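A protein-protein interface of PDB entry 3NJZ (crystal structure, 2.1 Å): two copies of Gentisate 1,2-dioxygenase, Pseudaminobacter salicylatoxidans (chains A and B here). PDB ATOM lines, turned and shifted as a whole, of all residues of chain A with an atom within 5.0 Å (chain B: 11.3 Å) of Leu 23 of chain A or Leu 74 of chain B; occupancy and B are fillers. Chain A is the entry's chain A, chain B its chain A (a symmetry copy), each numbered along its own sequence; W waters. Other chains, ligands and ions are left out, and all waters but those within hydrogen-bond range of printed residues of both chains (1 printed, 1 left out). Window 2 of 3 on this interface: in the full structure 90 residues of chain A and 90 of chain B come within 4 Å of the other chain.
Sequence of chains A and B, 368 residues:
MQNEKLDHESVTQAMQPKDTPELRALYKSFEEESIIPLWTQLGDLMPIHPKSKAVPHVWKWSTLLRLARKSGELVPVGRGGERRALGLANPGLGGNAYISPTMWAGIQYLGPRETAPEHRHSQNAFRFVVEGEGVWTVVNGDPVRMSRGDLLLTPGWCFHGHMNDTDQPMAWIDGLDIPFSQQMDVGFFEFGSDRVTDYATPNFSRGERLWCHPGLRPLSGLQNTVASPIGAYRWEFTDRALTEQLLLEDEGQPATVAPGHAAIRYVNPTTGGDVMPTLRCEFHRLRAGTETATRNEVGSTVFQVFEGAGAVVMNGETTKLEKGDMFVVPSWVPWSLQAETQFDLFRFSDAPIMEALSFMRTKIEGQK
Pro 17 of chain A touches just these residues of chain B: Leu 74 and Val 75. No residue of chain B comes within 4 Å of Asp 19 of chain A. No residue of chain B comes within 4 Å of Thr 20 of chain A. Of chain B, only Leu 74 comes within 4 Å of Glu 22 of chain A. Leu 23 of chain A touches one residue of chain B. No residue of chain B comes within 4 Å of Ala 25 of chain A. Of the printed residues of chain B, Leu 26 of chain A touches Lys 70 and Ser 71. No residue of chain B comes within 4 Å of Tyr 27 of chain A. Ala 68 of chain B touches none of the printed residues of chain A. Printed residues of chain A within 4 Å of Lys 70 of chain B: Leu 26 (3.5 Å). Of the printed residues of chain A, Ser 71 of chain B touches Leu 26 (3.6 Å). Leu 74 of chain B touches just these residues of chain A: Pro 17 (3.3 Å), Glu 22 (3.7 Å) and Leu 23 (3.9 Å). Of the printed residues of chain A, Val 75 of chain B touches Pro 17 (3.9 Å). Arg 83 of chain B touches none of the printed residues of chain A. The nearest residue of chain A that does not touch Leu 74 of chain B is Leu 26 of chain A (4.2 Å). The nearest printed residue of chain A that does not touch Lys 70 of chain B is Glu 22 of chain A (5.5 Å).
Water W1 lies within hydrogen-bond range of O of Lys 18 of chain A (3.0 Å) and O of Leu 74 of chain B (3.4 Å).
O of Ser 71 of chain B lies within hydrogen-bond range of NE of Arg 84 of chain B, at 3.3 Å. O of Leu 67 of chain B sits at hydrogen-bond distance from OG of Ser 71 of chain B, 2.7 Å away. The side-chain amino group (NZ) of Lys 70 of chain B lies within salt-bridge range of the side-chain carboxylate (OE2) of Glu 73 of chain B (3.4 Å). NH2 of Arg 84 of chain B sits at hydrogen-bond distance from O of Val 75 of chain B. The side-chain hydroxyl of Thr 20 of chain A sits close to the backbone NH of Glu 22 of chain A. The backbone NH (N) of Leu 23 of chain A sits at hydrogen-bond distance from the side-chain hydroxyl (OG1) of Thr 20 of chain A, at 3.1 Å.
Among the printed residues, merely in contact across the chains: Pro 17 of chain A with Leu 74 of chain B, Leu 26 of chain A with Lys 70 of chain B, Leu 26 of chain A with Ser 71 of chain B, Glu 22 of chain A with Leu 74 of chain B, Pro 17 of chain A with Val 75 of chain B and Leu 23 of chain A with Leu 74 of chain B.
No position is printed for both chains. Of the 6 pairs that touch across the chains among the printed residues, none has its exchanged pair printed and touching as well.
Of the 21 printed residues of chain B, 4 touch a printed residue of chain A. Printed residues of chain B that touch a printed residue of chain A: Lys 70, Ser 71, Leu 74 and Val 75. Hydrophobic or aromatic side chains of chain A that line the printed part of chain B: Pro 17 and Leu 26. Among the printed residues, no Asp or Glu carboxylate lies within 4 Å of a Lys or Arg side-chain nitrogen of the other chain.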
ATOM      1  N   PRO A  17       0.291  -7.506   1.698  1.00  0.00           N
ATOM      2  CA  PRO A  17      -0.843  -6.689   1.265  1.00  0.00           C
ATOM      3  C   PRO A  17      -2.190  -7.349   1.622  1.00  0.00           C
ATOM      4  O   PRO A  17      -2.256  -8.560   1.823  1.00  0.00           O
ATOM      5  CB  PRO A  17      -0.667  -6.625  -0.249  1.00  0.00           C
ATOM      6  CG  PRO A  17       0.077  -7.885  -0.588  1.00  0.00           C
ATOM      7  CD  PRO A  17       0.883  -8.295   0.612  1.00  0.00           C
ATOM      8  N   LYS A  18      -3.254  -6.559   1.691  1.00  0.00           N
ATOM      9  CA  LYS A  18      -4.586  -7.130   1.893  1.00  0.00           C
ATOM     10  C   LYS A  18      -4.959  -7.963   0.675  1.00  0.00           C
ATOM     11  O   LYS A  18      -4.787  -7.516  -0.463  1.00  0.00           O
ATOM     12  CB  LYS A  18      -5.609  -6.031   2.164  1.00  0.00           C
ATOM     13  CG  LYS A  18      -5.137  -5.083   3.245  1.00  0.00           C
ATOM     14  CD  LYS A  18      -6.269  -4.525   4.076  1.00  0.00           C
ATOM     15  CE  LYS A  18      -6.894  -3.305   3.444  1.00  0.00           C
ATOM     16  NZ  LYS A  18      -7.444  -2.449   4.550  1.00  0.00           N
ATOM     17  N   ASP A  19      -5.443  -9.174   0.914  1.00  0.00           N
ATOM     18  CA  ASP A  19      -5.766 -10.095  -0.179  1.00  0.00           C
ATOM     19  C   ASP A  19      -7.141  -9.830  -0.810  1.00  0.00           C
ATOM     20  O   ASP A  19      -8.144 -10.423  -0.442  1.00  0.00           O
ATOM     21  CB  ASP A  19      -5.595 -11.534   0.293  1.00  0.00           C
ATOM     22  CG  ASP A  19      -5.791 -12.544  -0.816  1.00  0.00           C
ATOM     23  OD1 ASP A  19      -5.839 -12.149  -2.010  1.00  0.00           O
ATOM     24  OD2 ASP A  19      -5.905 -13.748  -0.485  1.00  0.00           O
ATOM     25  N   THR A  20      -7.161  -8.917  -1.767  1.00  0.00           N
ATOM     26  CA  THR A  20      -8.386  -8.429  -2.393  1.00  0.00           C
ATOM     27  C   THR A  20      -8.386  -8.765  -3.876  1.00  0.00           C
ATOM     28  O   THR A  20      -7.335  -9.158  -4.425  1.00  0.00           O
ATOM     29  CB  THR A  20      -8.473  -6.900  -2.286  1.00  0.00           C
ATOM     30  OG1 THR A  20      -7.352  -6.314  -2.956  1.00  0.00           O
ATOM     31  CG2 THR A  20      -8.491  -6.433  -0.796  1.00  0.00           C
ATOM     32  N   PRO A  21      -9.554  -8.606  -4.550  1.00  0.00           N
ATOM     33  CA  PRO A  21      -9.506  -8.900  -5.982  1.00  0.00           C
ATOM     34  C   PRO A  21      -8.550  -7.951  -6.699  1.00  0.00           C
ATOM     35  O   PRO A  21      -7.990  -8.331  -7.708  1.00  0.00           O
ATOM     36  CB  PRO A  21     -10.946  -8.675  -6.465  1.00  0.00           C
ATOM     37  CG  PRO A  21     -11.816  -8.606  -5.214  1.00  0.00           C
ATOM     38  CD  PRO A  21     -10.928  -8.358  -4.043  1.00  0.00           C
ATOM     39  N   GLU A  22      -8.363  -6.737  -6.183  1.00  0.00           N
ATOM     40  CA  GLU A  22      -7.476  -5.771  -6.843  1.00  0.00           C
ATOM     41  C   GLU A  22      -6.029  -6.220  -6.724  1.00  0.00           C
ATOM     42  O   GLU A  22      -5.259  -6.065  -7.671  1.00  0.00           O
ATOM     43  CB  GLU A  22      -7.621  -4.351  -6.280  1.00  0.00           C
ATOM     44  CG  GLU A  22      -8.957  -3.665  -6.627  1.00  0.00           C
ATOM     45  CD  GLU A  22     -10.158  -4.135  -5.766  1.00  0.00           C
ATOM     46  OE1 GLU A  22     -10.001  -4.887  -4.769  1.00  0.00           O
ATOM     47  OE2 GLU A  22     -11.289  -3.744  -6.124  1.00  0.00           O
ATOM     48  N   LEU A  23      -5.690  -6.799  -5.568  1.00  0.00           N
ATOM     49  CA  LEU A  23      -4.355  -7.318  -5.337  1.00  0.00           C
ATOM     50  C   LEU A  23      -4.075  -8.538  -6.232  1.00  0.00           C
ATOM     51  O   LEU A  23      -3.032  -8.607  -6.886  1.00  0.00           O
ATOM     52  CB  LEU A  23      -4.100  -7.640  -3.861  1.00  0.00           C
ATOM     53  CG  LEU A  23      -2.659  -8.167  -3.720  1.00  0.00           C
ATOM     54  CD1 LEU A  23      -1.632  -7.018  -3.758  1.00  0.00           C
ATOM     55  CD2 LEU A  23      -2.474  -9.062  -2.512  1.00  0.00           C
ATOM     56  N   ARG A  24      -5.001  -9.496  -6.271  1.00  0.00           N
ATOM     57  CA  ARG A  24      -4.848 -10.656  -7.151  1.00  0.00           C
ATOM     58  C   ARG A  24      -4.763 -10.236  -8.615  1.00  0.00           C
ATOM     59  O   ARG A  24      -4.031 -10.855  -9.377  1.00  0.00           O
ATOM     60  CB  ARG A  24      -5.958 -11.702  -6.925  1.00  0.00           C
ATOM     61  CG  ARG A  24      -5.956 -12.197  -5.501  1.00  0.00           C
ATOM     62  CD  ARG A  24      -6.933 -13.330  -5.224  1.00  0.00           C
ATOM     63  NE  ARG A  24      -8.335 -12.923  -5.302  1.00  0.00           N
ATOM     64  CZ  ARG A  24      -9.077 -12.433  -4.298  1.00  0.00           C
ATOM     65  NH1 ARG A  24      -8.572 -12.221  -3.076  1.00  0.00           N
ATOM     66  NH2 ARG A  24     -10.346 -12.124  -4.537  1.00  0.00           N
ATOM     67  N   ALA A  25      -5.493  -9.193  -9.013  1.00  0.00           N
ATOM     68  CA  ALA A  25      -5.406  -8.729 -10.384  1.00  0.00           C
ATOM     69  C   ALA A  25      -4.031  -8.096 -10.629  1.00  0.00           C
ATOM     70  O   ALA A  25      -3.511  -8.184 -11.739  1.00  0.00           O
ATOM     71  CB  ALA A  25      -6.537  -7.731 -10.735  1.00  0.00           C
ATOM     72  N   LEU A  26      -3.469  -7.441  -9.604  1.00  0.00           N
ATOM     73  CA  LEU A  26      -2.142  -6.864  -9.719  1.00  0.00           C
ATOM     74  C   LEU A  26      -1.110  -7.987  -9.924  1.00  0.00           C
ATOM     75  O   LEU A  26      -0.261  -7.892 -10.805  1.00  0.00           O
ATOM     76  CB  LEU A  26      -1.774  -5.948  -8.531  1.00  0.00           C
ATOM     77  CG  LEU A  26      -0.344  -5.372  -8.516  1.00  0.00           C
ATOM     78  CD1 LEU A  26      -0.236  -4.317  -9.585  1.00  0.00           C
ATOM     79  CD2 LEU A  26       0.076  -4.778  -7.156  1.00  0.00           C
ATOM     80  N   TYR A  27      -1.220  -9.057  -9.141  1.00  0.00           N
ATOM     81  CA  TYR A  27      -0.275 -10.176  -9.235  1.00  0.00           C
ATOM     82  C   TYR A  27      -0.389 -10.910 -10.586  1.00  0.00           C
ATOM     83  O   TYR A  27       0.617 -11.373 -11.137  1.00  0.00           O
ATOM     84  CB  TYR A  27      -0.469 -11.140  -8.064  1.00  0.00           C
ATOM     85  CG  TYR A  27       0.120 -10.644  -6.756  1.00  0.00           C
ATOM     86  CD1 TYR A  27       0.592  -9.341  -6.632  1.00  0.00           C
ATOM     87  CD2 TYR A  27       0.175 -11.472  -5.629  1.00  0.00           C
ATOM     88  CE1 TYR A  27       1.117  -8.874  -5.456  1.00  0.00           C
ATOM     89  CE2 TYR A  27       0.722 -11.004  -4.415  1.00  0.00           C
ATOM     90  CZ  TYR A  27       1.177  -9.711  -4.349  1.00  0.00           C
ATOM     91  OH  TYR A  27       1.736  -9.229  -3.203  1.00  0.00           O
ATOM     92  N   LEU B  65       5.876   1.566 -14.954  1.00  0.00           N
ATOM     93  CA  LEU B  65       5.298   2.629 -14.125  1.00  0.00           C
ATOM     94  C   LEU B  65       3.874   2.326 -13.604  1.00  0.00           C
ATOM     95  O   LEU B  65       3.578   2.548 -12.404  1.00  0.00           O
ATOM     96  CB  LEU B  65       5.271   3.934 -14.898  1.00  0.00           C
ATOM     97  CG  LEU B  65       6.437   4.874 -14.619  1.00  0.00           C
ATOM     98  CD1 LEU B  65       6.145   6.220 -15.271  1.00  0.00           C
ATOM     99  CD2 LEU B  65       6.679   5.045 -13.098  1.00  0.00           C
ATOM    100  N   ARG B  66       3.016   1.832 -14.499  1.00  0.00           N
ATOM    101  CA  ARG B  66       1.641   1.469 -14.145  1.00  0.00           C
ATOM    102  C   ARG B  66       1.650   0.453 -13.004  1.00  0.00           C
ATOM    103  O   ARG B  66       0.975   0.642 -11.990  1.00  0.00           O
ATOM    104  CB  ARG B  66       0.897   0.880 -15.356  1.00  0.00           C
ATOM    105  CG  ARG B  66      -0.602   0.649 -15.117  1.00  0.00           C
ATOM    106  CD  ARG B  66      -1.316  -0.059 -16.299  1.00  0.00           C
ATOM    107  NE  ARG B  66      -1.146  -1.516 -16.283  1.00  0.00           N
ATOM    108  CZ  ARG B  66      -0.570  -2.225 -17.252  1.00  0.00           C
ATOM    109  NH1 ARG B  66      -0.110  -1.628 -18.342  1.00  0.00           N
ATOM    110  NH2 ARG B  66      -0.468  -3.543 -17.137  1.00  0.00           N
ATOM    111  N   LEU B  67       2.419  -0.626 -13.180  1.00  0.00           N
ATOM    112  CA  LEU B  67       2.524  -1.701 -12.188  1.00  0.00           C
ATOM    113  C   LEU B  67       3.180  -1.246 -10.884  1.00  0.00           C
ATOM    114  O   LEU B  67       2.793  -1.697  -9.789  1.00  0.00           O
ATOM    115  CB  LEU B  67       3.289  -2.907 -12.764  1.00  0.00           C
ATOM    116  CG  LEU B  67       2.716  -3.566 -14.030  1.00  0.00           C
ATOM    117  CD1 LEU B  67       3.633  -4.708 -14.524  1.00  0.00           C
ATOM    118  CD2 LEU B  67       1.321  -4.079 -13.793  1.00  0.00           C
ATOM    119  N   ALA B  68       4.169  -0.364 -11.003  1.00  0.00           N
ATOM    120  CA  ALA B  68       4.851   0.141  -9.823  1.00  0.00           C
ATOM    121  C   ALA B  68       3.899   1.052  -9.028  1.00  0.00           C
ATOM    122  O   ALA B  68       3.825   0.954  -7.800  1.00  0.00           O
ATOM    123  CB  ALA B  68       6.129   0.883 -10.202  1.00  0.00           C
ATOM    124  N   ARG B  69       3.180   1.914  -9.746  1.00  0.00           N
ATOM    125  CA  ARG B  69       2.191   2.811  -9.130  1.00  0.00           C
ATOM    126  C   ARG B  69       1.075   2.037  -8.410  1.00  0.00           C
ATOM    127  O   ARG B  69       0.744   2.340  -7.261  1.00  0.00           O
ATOM    128  CB  ARG B  69       1.594   3.765 -10.157  1.00  0.00           C
ATOM    129  CG  ARG B  69       2.503   4.943 -10.453  1.00  0.00           C
ATOM    130  CD  ARG B  69       2.017   5.715 -11.660  1.00  0.00           C
ATOM    131  NE  ARG B  69       2.995   6.722 -12.091  1.00  0.00           N
ATOM    132  CZ  ARG B  69       3.019   7.271 -13.309  1.00  0.00           C
ATOM    133  NH1 ARG B  69       2.128   6.909 -14.226  1.00  0.00           N
ATOM    134  NH2 ARG B  69       3.944   8.177 -13.618  1.00  0.00           N
ATOM    135  N   LYS B  70       0.538   1.015  -9.070  1.00  0.00           N
ATOM    136  CA  LYS B  70      -0.492   0.215  -8.449  1.00  0.00           C
ATOM    137  C   LYS B  70       0.052  -0.493  -7.211  1.00  0.00           C
ATOM    138  O   LYS B  70      -0.669  -0.614  -6.208  1.00  0.00           O
ATOM    139  CB  LYS B  70      -1.138  -0.758  -9.455  1.00  0.00           C
ATOM    140  CG  LYS B  70      -2.309  -1.597  -8.887  1.00  0.00           C
ATOM    141  CD  LYS B  70      -3.480  -0.739  -8.324  1.00  0.00           C
ATOM    142  CE  LYS B  70      -4.252  -0.049  -9.453  1.00  0.00           C
ATOM    143  NZ  LYS B  70      -5.599   0.401  -9.024  1.00  0.00           N
ATOM    144  N   SER B  71       1.310  -0.945  -7.270  1.00  0.00           N
ATOM    145  CA  SER B  71       1.980  -1.550  -6.110  1.00  0.00           C
ATOM    146  C   SER B  71       2.136  -0.553  -4.980  1.00  0.00           C
ATOM    147  O   SER B  71       2.102  -0.937  -3.828  1.00  0.00           O
ATOM    148  CB  SER B  71       3.364  -2.134  -6.452  1.00  0.00           C
ATOM    149  OG  SER B  71       3.292  -3.098  -7.489  1.00  0.00           O
ATOM    150  N   GLY B  72       2.308   0.723  -5.304  1.00  0.00           N
ATOM    151  CA  GLY B  72       2.423   1.754  -4.269  1.00  0.00           C
ATOM    152  C   GLY B  72       1.089   1.975  -3.561  1.00  0.00           C
ATOM    153  O   GLY B  72       1.066   2.429  -2.421  1.00  0.00           O
ATOM    154  N   GLU B  73      -0.006   1.627  -4.244  1.00  0.00           N
ATOM    155  CA  GLU B  73      -1.363   1.776  -3.709  1.00  0.00           C
ATOM    156  C   GLU B  73      -1.720   0.583  -2.828  1.00  0.00           C
ATOM    157  O   GLU B  73      -2.315   0.746  -1.768  1.00  0.00           O
ATOM    158  CB  GLU B  73      -2.385   1.922  -4.858  1.00  0.00           C
ATOM    159  CG  GLU B  73      -3.773   2.387  -4.414  1.00  0.00           C
ATOM    160  CD  GLU B  73      -4.851   2.239  -5.495  1.00  0.00           C
ATOM    161  OE1 GLU B  73      -5.959   1.771  -5.132  1.00  0.00           O
ATOM    162  OE2 GLU B  73      -4.604   2.600  -6.684  1.00  0.00           O
ATOM    163  N   LEU B  74      -1.328  -0.614  -3.259  1.00  0.00           N
ATOM    164  CA  LEU B  74      -1.787  -1.850  -2.619  1.00  0.00           C
ATOM    165  C   LEU B  74      -0.819  -2.540  -1.671  1.00  0.00           C
ATOM    166  O   LEU B  74      -1.223  -3.394  -0.875  1.00  0.00           O
ATOM    167  CB  LEU B  74      -2.230  -2.853  -3.686  1.00  0.00           C
ATOM    168  CG  LEU B  74      -3.279  -2.356  -4.681  1.00  0.00           C
ATOM    169  CD1 LEU B  74      -3.588  -3.459  -5.663  1.00  0.00           C
ATOM    170  CD2 LEU B  74      -4.572  -1.860  -3.975  1.00  0.00           C
ATOM    171  N   VAL B  75       0.466  -2.214  -1.774  1.00  0.00           N
ATOM    172  CA  VAL B  75       1.456  -2.920  -0.984  1.00  0.00           C
ATOM    173  C   VAL B  75       2.256  -1.948  -0.132  1.00  0.00           C
ATOM    174  O   VAL B  75       2.954  -1.095  -0.669  1.00  0.00           O
ATOM    175  CB  VAL B  75       2.404  -3.753  -1.868  1.00  0.00           C
ATOM    176  CG1 VAL B  75       3.450  -4.508  -1.006  1.00  0.00           C
ATOM    177  CG2 VAL B  75       1.620  -4.712  -2.734  1.00  0.00           C
ATOM    178  N   PRO B  76       2.182  -2.096   1.207  1.00  0.00           N
ATOM    179  CA  PRO B  76       3.040  -1.259   2.053  1.00  0.00           C
ATOM    180  C   PRO B  76       4.506  -1.739   1.986  1.00  0.00           C
ATOM    181  O   PRO B  76       4.766  -2.935   1.787  1.00  0.00           O
ATOM    182  CB  PRO B  76       2.462  -1.439   3.459  1.00  0.00           C
ATOM    183  CG  PRO B  76       1.718  -2.756   3.439  1.00  0.00           C
ATOM    184  CD  PRO B  76       1.539  -3.192   1.965  1.00  0.00           C
ATOM    185  N   VAL B  77       5.438  -0.786   2.108  1.00  0.00           N
ATOM    186  CA  VAL B  77       6.867  -1.077   2.132  1.00  0.00           C
ATOM    187  C   VAL B  77       7.310  -1.151   3.603  1.00  0.00           C
ATOM    188  O   VAL B  77       6.732  -0.487   4.470  1.00  0.00           O
ATOM    189  CB  VAL B  77       7.681  -0.005   1.347  1.00  0.00           C
ATOM    190  CG1 VAL B  77       7.570   1.360   2.026  1.00  0.00           C
ATOM    191  CG2 VAL B  77       9.120  -0.413   1.192  1.00  0.00           C
ATOM    192  N   GLY B  78       8.320  -1.970   3.881  1.00  0.00           N
ATOM    193  CA  GLY B  78       8.824  -2.090   5.240  1.00  0.00           C
ATOM    194  C   GLY B  78       9.607  -3.362   5.438  1.00  0.00           C
ATOM    195  O   GLY B  78       9.977  -4.039   4.457  1.00  0.00           O
ATOM    196  N   ARG B  83      11.739  -3.956   0.283  1.00  0.00           N
ATOM    197  CA  ARG B  83      11.687  -3.008  -0.829  1.00  0.00           C
ATOM    198  C   ARG B  83      10.440  -3.280  -1.664  1.00  0.00           C
ATOM    199  O   ARG B  83      10.095  -4.418  -1.887  1.00  0.00           O
ATOM    200  CB  ARG B  83      12.953  -3.149  -1.708  1.00  0.00           C
ATOM    201  CG  ARG B  83      14.303  -3.038  -0.941  1.00  0.00           C
ATOM    202  CD  ARG B  83      14.522  -1.623  -0.420  1.00  0.00           C
ATOM    203  NE  ARG B  83      15.831  -1.411   0.202  1.00  0.00           N
ATOM    204  CZ  ARG B  83      16.059  -1.392   1.522  1.00  0.00           C
ATOM    205  NH1 ARG B  83      15.054  -1.601   2.384  1.00  0.00           N
ATOM    206  NH2 ARG B  83      17.290  -1.138   1.989  1.00  0.00           N
ATOM    207  N   ARG B  84       9.750  -2.223  -2.086  1.00  0.00           N
ATOM    208  CA  ARG B  84       8.717  -2.340  -3.112  1.00  0.00           C
ATOM    209  C   ARG B  84       9.413  -2.278  -4.481  1.00  0.00           C
ATOM    210  O   ARG B  84       9.375  -1.262  -5.197  1.00  0.00           O
ATOM    211  CB  ARG B  84       7.660  -1.248  -2.959  1.00  0.00           C
ATOM    212  CG  ARG B  84       6.409  -1.441  -3.810  1.00  0.00           C
ATOM    213  CD  ARG B  84       5.507  -0.187  -3.722  1.00  0.00           C
ATOM    214  NE  ARG B  84       4.897   0.036  -2.390  1.00  0.00           N
ATOM    215  CZ  ARG B  84       5.207   1.038  -1.562  1.00  0.00           C
ATOM    216  NH1 ARG B  84       6.136   1.934  -1.891  1.00  0.00           N
ATOM    217  NH2 ARG B  84       4.591   1.156  -0.395  1.00  0.00           N
ATOM    218  N   LEU B  86      10.130  -4.358  -8.160  1.00  0.00           N
ATOM    219  CA  LEU B  86       9.618  -5.335  -9.139  1.00  0.00           C
ATOM    220  C   LEU B  86      10.748  -5.744 -10.075  1.00  0.00           C
ATOM    221  O   LEU B  86      11.239  -4.910 -10.836  1.00  0.00           O
ATOM    222  CB  LEU B  86       8.473  -4.711  -9.962  1.00  0.00           C
ATOM    223  CG  LEU B  86       7.281  -4.209  -9.131  1.00  0.00           C
ATOM    224  CD1 LEU B  86       6.271  -3.426  -9.931  1.00  0.00           C
ATOM    225  CD2 LEU B  86       6.613  -5.402  -8.500  1.00  0.00           C
ATOM    226  N   TYR B 109       9.689   1.678  -6.254  1.00  0.00           N
ATOM    227  CA  TYR B 109       8.762   2.799  -6.056  1.00  0.00           C
ATOM    228  C   TYR B 109       8.695   3.130  -4.573  1.00  0.00           C
ATOM    229  O   TYR B 109       8.456   2.253  -3.733  1.00  0.00           O
ATOM    230  CB  TYR B 109       7.389   2.406  -6.598  1.00  0.00           C
ATOM    231  CG  TYR B 109       6.294   3.469  -6.559  1.00  0.00           C
ATOM    232  CD1 TYR B 109       6.030   4.277  -7.686  1.00  0.00           C
ATOM    233  CD2 TYR B 109       5.491   3.646  -5.415  1.00  0.00           C
ATOM    234  CE1 TYR B 109       5.016   5.237  -7.672  1.00  0.00           C
ATOM    235  CE2 TYR B 109       4.455   4.606  -5.401  1.00  0.00           C
ATOM    236  CZ  TYR B 109       4.234   5.389  -6.541  1.00  0.00           C
ATOM    237  OH  TYR B 109       3.220   6.337  -6.545  1.00  0.00           O
ATOM    238  N   GLY B 111       6.738   5.858  -2.159  1.00  0.00           N
ATOM    239  CA  GLY B 111       5.674   6.852  -2.130  1.00  0.00           C
ATOM    240  C   GLY B 111       5.989   8.005  -1.181  1.00  0.00           C
ATOM    241  O   GLY B 111       6.991   7.976  -0.479  1.00  0.00           O
ATOM    242  N   PRO B 112       5.117   9.037  -1.150  1.00  0.00           N
ATOM    243  CA  PRO B 112       5.287  10.194  -0.242  1.00  0.00           C
ATOM    244  C   PRO B 112       5.717   9.801   1.181  1.00  0.00           C
ATOM    245  O   PRO B 112       5.082   8.954   1.793  1.00  0.00           O
ATOM    246  CB  PRO B 112       3.881  10.791  -0.198  1.00  0.00           C
ATOM    247  CG  PRO B 112       3.291  10.476  -1.552  1.00  0.00           C
ATOM    248  CD  PRO B 112       3.887   9.137  -1.969  1.00  0.00           C
ATOM    249  N   GLU B 114       7.640   7.873   2.687  1.00  0.00           N
ATOM    250  CA  GLU B 114       7.961   6.508   3.110  1.00  0.00           C
ATOM    251  C   GLU B 114       9.444   6.305   3.351  1.00  0.00           C
ATOM    252  O   GLU B 114      10.283   6.966   2.741  1.00  0.00           O
ATOM    253  CB  GLU B 114       7.496   5.495   2.071  1.00  0.00           C
ATOM    254  CG  GLU B 114       5.983   5.402   1.874  1.00  0.00           C
ATOM    255  CD  GLU B 114       5.658   4.372   0.808  1.00  0.00           C
ATOM    256  OE1 GLU B 114       6.515   4.113  -0.080  1.00  0.00           O
ATOM    257  OE2 GLU B 114       4.560   3.805   0.868  1.00  0.00           O
HETATM  258  O   HOH W   1      -4.339  -4.738  -1.364  1.00  0.00           O
